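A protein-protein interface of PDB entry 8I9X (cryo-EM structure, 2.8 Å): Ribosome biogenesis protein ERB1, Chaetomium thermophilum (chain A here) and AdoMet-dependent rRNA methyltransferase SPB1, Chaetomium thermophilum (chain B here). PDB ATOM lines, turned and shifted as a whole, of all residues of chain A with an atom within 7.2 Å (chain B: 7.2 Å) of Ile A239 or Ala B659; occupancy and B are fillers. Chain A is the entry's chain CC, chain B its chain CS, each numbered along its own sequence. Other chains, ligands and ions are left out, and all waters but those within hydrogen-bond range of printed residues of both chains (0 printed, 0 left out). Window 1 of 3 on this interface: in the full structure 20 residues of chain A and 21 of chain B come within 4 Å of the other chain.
The guanidinium group (NH2) of Arg A240 is in salt-bridge range of the side-chain carboxylate (OE1) of Glu A237.
Among the printed residues, no Asp or Glu carboxylate lies within 4 Å of a Lys or Arg side-chain nitrogen of the other chain.
CB of Ala B663 touches CD1 of Leu A231, at 3.6 Å.
Leu A236 touches Ile B652.
CD2 of Leu A236 touches CD1 of Ile B654 (3.9 Å).
Glu A237 touches Ile B652 (OE2 to CD1, 3.2 Å).
CD2 of Leu A238 touches CD1 of Leu B676, 3.5 Å away.
Ile A239 touches Ala B659.
CD1 of Ile A239 touches CD2 of Leu B666, 3.8 Å away.
Arg A240 touches Ile B652.
CD1 of Leu B662 touches CG1 of Val A242 (3.7 Å).
Gln A243 touches Leu B662 (OE1 to CD1, 3.3 Å).
Ile A239 touches just these residues of chain B: Ala B659 and Leu B666.
Ala B659 touches just one residue of chain A: Ile A239.
Of the printed residues of chain A, Leu B666 touches Ile A239 (3.8 Å).
Of the printed residues of chain A, Ile B652 touches Leu A236 (3.6 Å), Glu A237 (3.2 Å) and Arg A240 (3.7 Å).
Of the printed residues of chain B, Val A242 touches Leu B662 (3.7 Å).
Printed residues of chain A within 4 Å of Leu B676: Leu A238 (3.5 Å).
Gln B665 touches none of the printed residues of chain A.
Ala B714 touches none of the printed residues of chain A.
The nearest residue of chain B that does not touch Ile A239 is Leu B676 (4.1 Å).
The nearest residue of chain A that does not touch Ala B659 is Gln A243 (4.1 Å).
The nearest printed residue of chain B that does not touch Leu A236 is Asp B653 (5.9 Å).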
ATOM      1  N   LEU A 231      17.269  -0.683  23.054  1.00  0.00           N
ATOM      2  CA  LEU A 231      16.315  -0.755  24.151  1.00  0.00           C
ATOM      3  C   LEU A 231      16.365   0.523  24.978  1.00  0.00           C
ATOM      4  O   LEU A 231      17.431   1.111  25.181  1.00  0.00           O
ATOM      5  CB  LEU A 231      16.612  -1.959  25.039  1.00  0.00           C
ATOM      6  CG  LEU A 231      16.526  -3.346  24.405  1.00  0.00           C
ATOM      7  CD1 LEU A 231      17.018  -4.384  25.394  1.00  0.00           C
ATOM      8  CD2 LEU A 231      15.115  -3.664  23.950  1.00  0.00           C
ATOM      9  N   ARG A 233      15.359   2.839  28.588  1.00  0.00           N
ATOM     10  CA  ARG A 233      15.540   2.640  30.023  1.00  0.00           C
ATOM     11  C   ARG A 233      14.447   1.755  30.609  1.00  0.00           C
ATOM     12  O   ARG A 233      14.742   0.799  31.335  1.00  0.00           O
ATOM     13  CB  ARG A 233      15.568   3.990  30.736  1.00  0.00           C
ATOM     14  CG  ARG A 233      16.709   4.896  30.320  1.00  0.00           C
ATOM     15  CD  ARG A 233      18.031   4.295  30.753  1.00  0.00           C
ATOM     16  NE  ARG A 233      18.113   4.221  32.207  1.00  0.00           N
ATOM     17  CZ  ARG A 233      18.977   3.472  32.876  1.00  0.00           C
ATOM     18  NH1 ARG A 233      19.858   2.709  32.252  1.00  0.00           N
ATOM     19  NH2 ARG A 233      18.956   3.487  34.206  1.00  0.00           N
ATOM     20  N   ASP A 234      13.184   2.058  30.311  1.00  0.00           N
ATOM     21  CA  ASP A 234      12.088   1.273  30.862  1.00  0.00           C
ATOM     22  C   ASP A 234      12.095  -0.157  30.343  1.00  0.00           C
ATOM     23  O   ASP A 234      11.806  -1.090  31.102  1.00  0.00           O
ATOM     24  CB  ASP A 234      10.748   1.947  30.559  1.00  0.00           C
ATOM     25  CG  ASP A 234      10.516   2.149  29.076  1.00  0.00           C
ATOM     26  OD1 ASP A 234      11.458   1.929  28.288  1.00  0.00           O
ATOM     27  OD2 ASP A 234       9.388   2.529  28.697  1.00  0.00           O
ATOM     28  N   GLU A 235      12.431  -0.355  29.067  1.00  0.00           N
ATOM     29  CA  GLU A 235      12.520  -1.709  28.534  1.00  0.00           C
ATOM     30  C   GLU A 235      13.633  -2.506  29.204  1.00  0.00           C
ATOM     31  O   GLU A 235      13.436  -3.682  29.534  1.00  0.00           O
ATOM     32  CB  GLU A 235      12.724  -1.663  27.021  1.00  0.00           C
ATOM     33  CG  GLU A 235      11.590  -0.976  26.279  1.00  0.00           C
ATOM     34  CD  GLU A 235      11.441  -1.459  24.852  1.00  0.00           C
ATOM     35  OE1 GLU A 235      12.451  -1.886  24.258  1.00  0.00           O
ATOM     36  OE2 GLU A 235      10.310  -1.412  24.323  1.00  0.00           O
ATOM     37  N   LEU A 236      14.800  -1.892  29.420  1.00  0.00           N
ATOM     38  CA  LEU A 236      15.870  -2.588  30.127  1.00  0.00           C
ATOM     39  C   LEU A 236      15.480  -2.897  31.566  1.00  0.00           C
ATOM     40  O   LEU A 236      15.806  -3.976  32.078  1.00  0.00           O
ATOM     41  CB  LEU A 236      17.155  -1.764  30.088  1.00  0.00           C
ATOM     42  CG  LEU A 236      17.858  -1.686  28.734  1.00  0.00           C
ATOM     43  CD1 LEU A 236      18.677  -0.412  28.624  1.00  0.00           C
ATOM     44  CD2 LEU A 236      18.733  -2.908  28.519  1.00  0.00           C
ATOM     45  N   GLU A 237      14.778  -1.972  32.228  1.00  0.00           N
ATOM     46  CA  GLU A 237      14.266  -2.250  33.564  1.00  0.00           C
ATOM     47  C   GLU A 237      13.319  -3.439  33.557  1.00  0.00           C
ATOM     48  O   GLU A 237      13.365  -4.278  34.463  1.00  0.00           O
ATOM     49  CB  GLU A 237      13.547  -1.021  34.125  1.00  0.00           C
ATOM     50  CG  GLU A 237      14.434   0.184  34.395  1.00  0.00           C
ATOM     51  CD  GLU A 237      15.428  -0.053  35.513  1.00  0.00           C
ATOM     52  OE1 GLU A 237      15.103  -0.816  36.446  1.00  0.00           O
ATOM     53  OE2 GLU A 237      16.529   0.534  35.464  1.00  0.00           O
ATOM     54  N   LEU A 238      12.451  -3.525  32.549  1.00  0.00           N
ATOM     55  CA  LEU A 238      11.510  -4.635  32.480  1.00  0.00           C
ATOM     56  C   LEU A 238      12.226  -5.957  32.232  1.00  0.00           C
ATOM     57  O   LEU A 238      11.851  -6.987  32.803  1.00  0.00           O
ATOM     58  CB  LEU A 238      10.469  -4.370  31.396  1.00  0.00           C
ATOM     59  CG  LEU A 238       9.369  -5.416  31.276  1.00  0.00           C
ATOM     60  CD1 LEU A 238       8.555  -5.476  32.555  1.00  0.00           C
ATOM     61  CD2 LEU A 238       8.488  -5.083  30.099  1.00  0.00           C
ATOM     62  N   ILE A 239      13.253  -5.953  31.379  1.00  0.00           N
ATOM     63  CA  ILE A 239      14.033  -7.171  31.171  1.00  0.00           C
ATOM     64  C   ILE A 239      14.723  -7.591  32.463  1.00  0.00           C
ATOM     65  O   ILE A 239      14.770  -8.781  32.800  1.00  0.00           O
ATOM     66  CB  ILE A 239      15.042  -6.992  30.021  1.00  0.00           C
ATOM     67  CG1 ILE A 239      14.352  -6.482  28.753  1.00  0.00           C
ATOM     68  CG2 ILE A 239      15.763  -8.299  29.739  1.00  0.00           C
ATOM     69  CD1 ILE A 239      13.081  -7.226  28.391  1.00  0.00           C
ATOM     70  N   ARG A 240      15.277  -6.626  33.201  1.00  0.00           N
ATOM     71  CA  ARG A 240      15.850  -6.925  34.511  1.00  0.00           C
ATOM     72  C   ARG A 240      14.823  -7.553  35.444  1.00  0.00           C
ATOM     73  O   ARG A 240      15.116  -8.545  36.126  1.00  0.00           O
ATOM     74  CB  ARG A 240      16.405  -5.649  35.134  1.00  0.00           C
ATOM     75  CG  ARG A 240      17.072  -5.855  36.473  1.00  0.00           C
ATOM     76  CD  ARG A 240      17.590  -4.537  37.001  1.00  0.00           C
ATOM     77  NE  ARG A 240      16.497  -3.601  37.231  1.00  0.00           N
ATOM     78  CZ  ARG A 240      15.743  -3.576  38.321  1.00  0.00           C
ATOM     79  NH1 ARG A 240      15.936  -4.426  39.315  1.00  0.00           N
ATOM     80  NH2 ARG A 240      14.766  -2.677  38.413  1.00  0.00           N
ATOM     81  N   LYS A 241      13.626  -6.970  35.509  1.00  0.00           N
ATOM     82  CA  LYS A 241      12.594  -7.488  36.399  1.00  0.00           C
ATOM     83  C   LYS A 241      12.178  -8.898  36.002  1.00  0.00           C
ATOM     84  O   LYS A 241      11.928  -9.740  36.868  1.00  0.00           O
ATOM     85  CB  LYS A 241      11.387  -6.551  36.413  1.00  0.00           C
ATOM     86  CG  LYS A 241      11.658  -5.192  37.038  1.00  0.00           C
ATOM     87  CD  LYS A 241      10.401  -4.334  37.065  1.00  0.00           C
ATOM     88  CE  LYS A 241      10.692  -2.947  37.616  1.00  0.00           C
ATOM     89  NZ  LYS A 241      11.051  -2.987  39.061  1.00  0.00           N
ATOM     90  N   VAL A 242      12.096  -9.174  34.702  1.00  0.00           N
ATOM     91  CA  VAL A 242      11.728 -10.516  34.261  1.00  0.00           C
ATOM     92  C   VAL A 242      12.833 -11.516  34.586  1.00  0.00           C
ATOM     93  O   VAL A 242      12.558 -12.641  35.017  1.00  0.00           O
ATOM     94  CB  VAL A 242      11.387 -10.510  32.760  1.00  0.00           C
ATOM     95  CG1 VAL A 242      11.174 -11.927  32.258  1.00  0.00           C
ATOM     96  CG2 VAL A 242      10.147  -9.674  32.509  1.00  0.00           C
ATOM     97  N   GLN A 243      14.094 -11.125  34.398  1.00  0.00           N
ATOM     98  CA  GLN A 243      15.205 -12.025  34.681  1.00  0.00           C
ATOM     99  C   GLN A 243      15.369 -12.328  36.163  1.00  0.00           C
ATOM    100  O   GLN A 243      15.690 -13.468  36.513  1.00  0.00           O
ATOM    101  CB  GLN A 243      16.505 -11.444  34.124  1.00  0.00           C
ATOM    102  CG  GLN A 243      16.735 -11.751  32.661  1.00  0.00           C
ATOM    103  CD  GLN A 243      16.672 -13.236  32.373  1.00  0.00           C
ATOM    104  OE1 GLN A 243      15.715 -13.719  31.769  1.00  0.00           O
ATOM    105  NE2 GLN A 243      17.694 -13.966  32.790  1.00  0.00           N
ATOM    106  N   GLN A 244      15.165 -11.350  37.044  1.00  0.00           N
ATOM    107  CA  GLN A 244      15.391 -11.590  38.465  1.00  0.00           C
ATOM    108  C   GLN A 244      14.141 -12.016  39.227  1.00  0.00           C
ATOM    109  O   GLN A 244      14.250 -12.814  40.162  1.00  0.00           O
ATOM    110  CB  GLN A 244      15.994 -10.346  39.128  1.00  0.00           C
ATOM    111  CG  GLN A 244      17.072  -9.674  38.298  1.00  0.00           C
ATOM    112  CD  GLN A 244      18.069  -8.912  39.143  1.00  0.00           C
ATOM    113  OE1 GLN A 244      17.697  -8.223  40.093  1.00  0.00           O
ATOM    114  NE2 GLN A 244      19.346  -9.030  38.803  1.00  0.00           N
ATOM    115  N   GLY A 245      12.965 -11.512  38.862  1.00  0.00           N
ATOM    116  CA  GLY A 245      11.723 -11.939  39.468  1.00  0.00           C
ATOM    117  C   GLY A 245      11.356 -11.259  40.768  1.00  0.00           C
ATOM    118  O   GLY A 245      10.288 -11.557  41.318  1.00  0.00           O
ATOM    119  N   ILE B 652      22.103  -1.079  33.683  1.00  0.00           N
ATOM    120  CA  ILE B 652      21.713  -2.445  33.355  1.00  0.00           C
ATOM    121  C   ILE B 652      22.479  -2.878  32.114  1.00  0.00           C
ATOM    122  O   ILE B 652      22.411  -2.221  31.069  1.00  0.00           O
ATOM    123  CB  ILE B 652      20.198  -2.557  33.131  1.00  0.00           C
ATOM    124  CG1 ILE B 652      19.444  -2.214  34.413  1.00  0.00           C
ATOM    125  CG2 ILE B 652      19.833  -3.953  32.659  1.00  0.00           C
ATOM    126  CD1 ILE B 652      17.961  -2.052  34.210  1.00  0.00           C
ATOM    127  N   ASP B 653      23.208  -3.982  32.228  1.00  0.00           N
ATOM    128  CA  ASP B 653      24.011  -4.515  31.136  1.00  0.00           C
ATOM    129  C   ASP B 653      23.594  -5.961  30.906  1.00  0.00           C
ATOM    130  O   ASP B 653      23.509  -6.744  31.858  1.00  0.00           O
ATOM    131  CB  ASP B 653      25.502  -4.415  31.460  1.00  0.00           C
ATOM    132  CG  ASP B 653      26.390  -4.760  30.276  1.00  0.00           C
ATOM    133  OD1 ASP B 653      27.353  -4.005  30.024  1.00  0.00           O
ATOM    134  OD2 ASP B 653      26.138  -5.776  29.596  1.00  0.00           O
ATOM    135  N   ILE B 654      23.334  -6.306  29.652  1.00  0.00           N
ATOM    136  CA  ILE B 654      22.944  -7.666  29.300  1.00  0.00           C
ATOM    137  C   ILE B 654      24.183  -8.447  28.885  1.00  0.00           C
ATOM    138  O   ILE B 654      24.758  -8.204  27.819  1.00  0.00           O
ATOM    139  CB  ILE B 654      21.893  -7.654  28.178  1.00  0.00           C
ATOM    140  CG1 ILE B 654      20.614  -6.968  28.656  1.00  0.00           C
ATOM    141  CG2 ILE B 654      21.614  -9.065  27.699  1.00  0.00           C
ATOM    142  CD1 ILE B 654      19.669  -6.597  27.540  1.00  0.00           C
ATOM    143  N   ILE B 655      24.586  -9.401  29.719  1.00  0.00           N
ATOM    144  CA  ILE B 655      25.758 -10.225  29.443  1.00  0.00           C
ATOM    145  C   ILE B 655      25.319 -11.677  29.341  1.00  0.00           C
ATOM    146  O   ILE B 655      26.151 -12.588  29.283  1.00  0.00           O
ATOM    147  CB  ILE B 655      26.837 -10.053  30.527  1.00  0.00           C
ATOM    148  CG1 ILE B 655      26.305 -10.509  31.886  1.00  0.00           C
ATOM    149  CG2 ILE B 655      27.295  -8.611  30.600  1.00  0.00           C
ATOM    150  CD1 ILE B 655      27.365 -10.593  32.958  1.00  0.00           C
ATOM    151  N   THR B 656      24.009 -11.899  29.311  1.00  0.00           N
ATOM    152  CA  THR B 656      23.429 -13.228  29.413  1.00  0.00           C
ATOM    153  C   THR B 656      22.612 -13.545  28.165  1.00  0.00           C
ATOM    154  O   THR B 656      21.901 -12.686  27.630  1.00  0.00           O
ATOM    155  CB  THR B 656      22.554 -13.333  30.671  1.00  0.00           C
ATOM    156  OG1 THR B 656      23.358 -13.083  31.830  1.00  0.00           O
ATOM    157  CG2 THR B 656      21.949 -14.709  30.795  1.00  0.00           C
ATOM    158  N   ALA B 657      22.727 -14.795  27.706  1.00  0.00           N
ATOM    159  CA  ALA B 657      22.033 -15.218  26.495  1.00  0.00           C
ATOM    160  C   ALA B 657      20.518 -15.168  26.652  1.00  0.00           C
ATOM    161  O   ALA B 657      19.824 -14.731  25.732  1.00  0.00           O
ATOM    162  CB  ALA B 657      22.480 -16.623  26.097  1.00  0.00           C
ATOM    163  N   GLU B 658      19.984 -15.613  27.793  1.00  0.00           N
ATOM    164  CA  GLU B 658      18.544 -15.512  28.021  1.00  0.00           C
ATOM    165  C   GLU B 658      18.059 -14.070  28.051  1.00  0.00           C
ATOM    166  O   GLU B 658      17.001 -13.767  27.481  1.00  0.00           O
ATOM    167  CB  GLU B 658      18.153 -16.211  29.327  1.00  0.00           C
ATOM    168  CG  GLU B 658      18.320 -17.725  29.331  1.00  0.00           C
ATOM    169  CD  GLU B 658      19.735 -18.173  29.624  1.00  0.00           C
ATOM    170  OE1 GLU B 658      20.592 -17.310  29.890  1.00  0.00           O
ATOM    171  OE2 GLU B 658      19.993 -19.395  29.587  1.00  0.00           O
ATOM    172  N   ALA B 659      18.799 -13.180  28.707  1.00  0.00           N
ATOM    173  CA  ALA B 659      18.437 -11.772  28.723  1.00  0.00           C
ATOM    174  C   ALA B 659      18.457 -11.159  27.332  1.00  0.00           C
ATOM    175  O   ALA B 659      17.543 -10.402  26.986  1.00  0.00           O
ATOM    176  CB  ALA B 659      19.376 -10.998  29.650  1.00  0.00           C
ATOM    177  N   MET B 660      19.460 -11.485  26.514  1.00  0.00           N
ATOM    178  CA  MET B 660      19.469 -10.966  25.152  1.00  0.00           C
ATOM    179  C   MET B 660      18.373 -11.598  24.301  1.00  0.00           C
ATOM    180  O   MET B 660      17.861 -10.955  23.380  1.00  0.00           O
ATOM    181  CB  MET B 660      20.842 -11.174  24.514  1.00  0.00           C
ATOM    182  CG  MET B 660      20.956 -10.605  23.111  1.00  0.00           C
ATOM    183  SD  MET B 660      21.087  -8.806  23.056  1.00  0.00           S
ATOM    184  CE  MET B 660      22.414  -8.508  24.216  1.00  0.00           C
ATOM    185  N   THR B 661      17.988 -12.842  24.595  1.00  0.00           N
ATOM    186  CA  THR B 661      16.861 -13.446  23.892  1.00  0.00           C
ATOM    187  C   THR B 661      15.566 -12.703  24.192  1.00  0.00           C
ATOM    188  O   THR B 661      14.784 -12.405  23.279  1.00  0.00           O
ATOM    189  CB  THR B 661      16.733 -14.920  24.271  1.00  0.00           C
ATOM    190  OG1 THR B 661      17.987 -15.580  24.062  1.00  0.00           O
ATOM    191  CG2 THR B 661      15.667 -15.593  23.426  1.00  0.00           C
ATOM    192  N   LEU B 662      15.324 -12.386  25.466  1.00  0.00           N
ATOM    193  CA  LEU B 662      14.155 -11.574  25.798  1.00  0.00           C
ATOM    194  C   LEU B 662      14.250 -10.180  25.194  1.00  0.00           C
ATOM    195  O   LEU B 662      13.229  -9.610  24.792  1.00  0.00           O
ATOM    196  CB  LEU B 662      13.967 -11.477  27.310  1.00  0.00           C
ATOM    197  CG  LEU B 662      13.617 -12.766  28.048  1.00  0.00           C
ATOM    198  CD1 LEU B 662      13.605 -12.511  29.538  1.00  0.00           C
ATOM    199  CD2 LEU B 662      12.274 -13.302  27.582  1.00  0.00           C
ATOM    200  N   ALA B 663      15.454  -9.610  25.137  1.00  0.00           N
ATOM    201  CA  ALA B 663      15.636  -8.322  24.480  1.00  0.00           C
ATOM    202  C   ALA B 663      15.257  -8.377  23.007  1.00  0.00           C
ATOM    203  O   ALA B 663      14.574  -7.476  22.513  1.00  0.00           O
ATOM    204  CB  ALA B 663      17.085  -7.861  24.630  1.00  0.00           C
ATOM    205  N   HIS B 664      15.692  -9.422  22.301  1.00  0.00           N
ATOM    206  CA  HIS B 664      15.305  -9.609  20.907  1.00  0.00           C
ATOM    207  C   HIS B 664      13.798  -9.770  20.768  1.00  0.00           C
ATOM    208  O   HIS B 664      13.186  -9.206  19.852  1.00  0.00           O
ATOM    209  CB  HIS B 664      16.024 -10.828  20.330  1.00  0.00           C
ATOM    210  CG  HIS B 664      17.419 -10.550  19.866  1.00  0.00           C
ATOM    211  ND1 HIS B 664      18.487 -10.454  20.730  1.00  0.00           N
ATOM    212  CD2 HIS B 664      17.926 -10.382  18.623  1.00  0.00           C
ATOM    213  CE1 HIS B 664      19.589 -10.216  20.041  1.00  0.00           C
ATOM    214  NE2 HIS B 664      19.275 -10.168  18.760  1.00  0.00           N
ATOM    215  N   GLN B 665      13.184 -10.551  21.658  1.00  0.00           N
ATOM    216  CA  GLN B 665      11.746 -10.770  21.605  1.00  0.00           C
ATOM    217  C   GLN B 665      10.947  -9.500  21.865  1.00  0.00           C
ATOM    218  O   GLN B 665       9.889  -9.323  21.255  1.00  0.00           O
ATOM    219  CB  GLN B 665      11.355 -11.863  22.599  1.00  0.00           C
ATOM    220  CG  GLN B 665      11.905 -13.228  22.224  1.00  0.00           C
ATOM    221  CD  GLN B 665      11.541 -14.308  23.216  1.00  0.00           C
ATOM    222  OE1 GLN B 665      10.921 -14.039  24.242  1.00  0.00           O
ATOM    223  NE2 GLN B 665      11.926 -15.542  22.915  1.00  0.00           N
ATOM    224  N   LEU B 666      11.415  -8.623  22.753  1.00  0.00           N
ATOM    225  CA  LEU B 666      10.797  -7.313  22.922  1.00  0.00           C
ATOM    226  C   LEU B 666      11.040  -6.387  21.740  1.00  0.00           C
ATOM    227  O   LEU B 666      10.134  -5.649  21.339  1.00  0.00           O
ATOM    228  CB  LEU B 666      11.298  -6.642  24.202  1.00  0.00           C
ATOM    229  CG  LEU B 666      10.287  -5.664  24.804  1.00  0.00           C
ATOM    230  CD1 LEU B 666       8.905  -6.284  24.885  1.00  0.00           C
ATOM    231  CD2 LEU B 666      10.750  -5.183  26.170  1.00  0.00           C
ATOM    232  N   LEU B 676       5.049  -9.396  28.891  1.00  0.00           N
ATOM    233  CA  LEU B 676       6.168  -9.666  29.789  1.00  0.00           C
ATOM    234  C   LEU B 676       5.763  -9.616  31.258  1.00  0.00           C
ATOM    235  O   LEU B 676       6.191 -10.471  32.035  1.00  0.00           O
ATOM    236  CB  LEU B 676       7.331  -8.713  29.528  1.00  0.00           C
ATOM    237  CG  LEU B 676       7.995  -8.892  28.167  1.00  0.00           C
ATOM    238  CD1 LEU B 676       9.035  -7.826  27.958  1.00  0.00           C
ATOM    239  CD2 LEU B 676       8.618 -10.268  28.071  1.00  0.00           C
ATOM    240  N   LYS B 708      14.848 -21.667  29.308  1.00  0.00           N
ATOM    241  CA  LYS B 708      14.255 -21.031  28.151  1.00  0.00           C
ATOM    242  C   LYS B 708      15.111 -21.295  26.920  1.00  0.00           C
ATOM    243  O   LYS B 708      16.342 -21.347  27.023  1.00  0.00           O
ATOM    244  CB  LYS B 708      14.113 -19.512  28.346  1.00  0.00           C
ATOM    245  CG  LYS B 708      12.956 -19.083  29.233  1.00  0.00           C
ATOM    246  CD  LYS B 708      13.352 -19.090  30.696  1.00  0.00           C
ATOM    247  CE  LYS B 708      14.349 -17.979  30.983  1.00  0.00           C
ATOM    248  NZ  LYS B 708      14.718 -17.905  32.422  1.00  0.00           N
ATOM    249  N   ILE B 710      17.340 -20.658  23.724  1.00  0.00           N
ATOM    250  CA  ILE B 710      18.230 -19.594  23.300  1.00  0.00           C
ATOM    251  C   ILE B 710      18.237 -19.558  21.779  1.00  0.00           C
ATOM    252  O   ILE B 710      18.163 -20.587  21.102  1.00  0.00           O
ATOM    253  CB  ILE B 710      19.658 -19.781  23.861  1.00  0.00           C
ATOM    254  CG1 ILE B 710      19.612 -19.933  25.379  1.00  0.00           C
ATOM    255  CG2 ILE B 710      20.550 -18.612  23.481  1.00  0.00           C
ATOM    256  CD1 ILE B 710      19.352 -18.639  26.098  1.00  0.00           C
ATOM    257  N   ALA B 714      20.733 -14.270  19.476  1.00  0.00           N
ATOM    258  CA  ALA B 714      21.101 -13.799  20.807  1.00  0.00           C
ATOM    259  C   ALA B 714      22.485 -14.294  21.207  1.00  0.00           C
ATOM    260  O   ALA B 714      23.275 -13.542  21.792  1.00  0.00           O
ATOM    261  CB  ALA B 714      20.056 -14.243  21.829  1.00  0.00           C
ATOM    262  N   ILE B 718      25.649 -11.839  22.047  1.00  0.00           N
ATOM    263  CA  ILE B 718      26.408 -11.899  23.292  1.00  0.00           C
ATOM    264  C   ILE B 718      27.890 -12.120  23.010  1.00  0.00           C
ATOM    265  O   ILE B 718      28.752 -11.470  23.617  1.00  0.00           O
ATOM    266  CB  ILE B 718      25.832 -12.986  24.216  1.00  0.00           C
ATOM    267  CG1 ILE B 718      24.434 -12.592  24.685  1.00  0.00           C
ATOM    268  CG2 ILE B 718      26.745 -13.220  25.407  1.00  0.00           C
ATOM    269  CD1 ILE B 718      24.408 -11.303  25.468  1.00  0.00           C
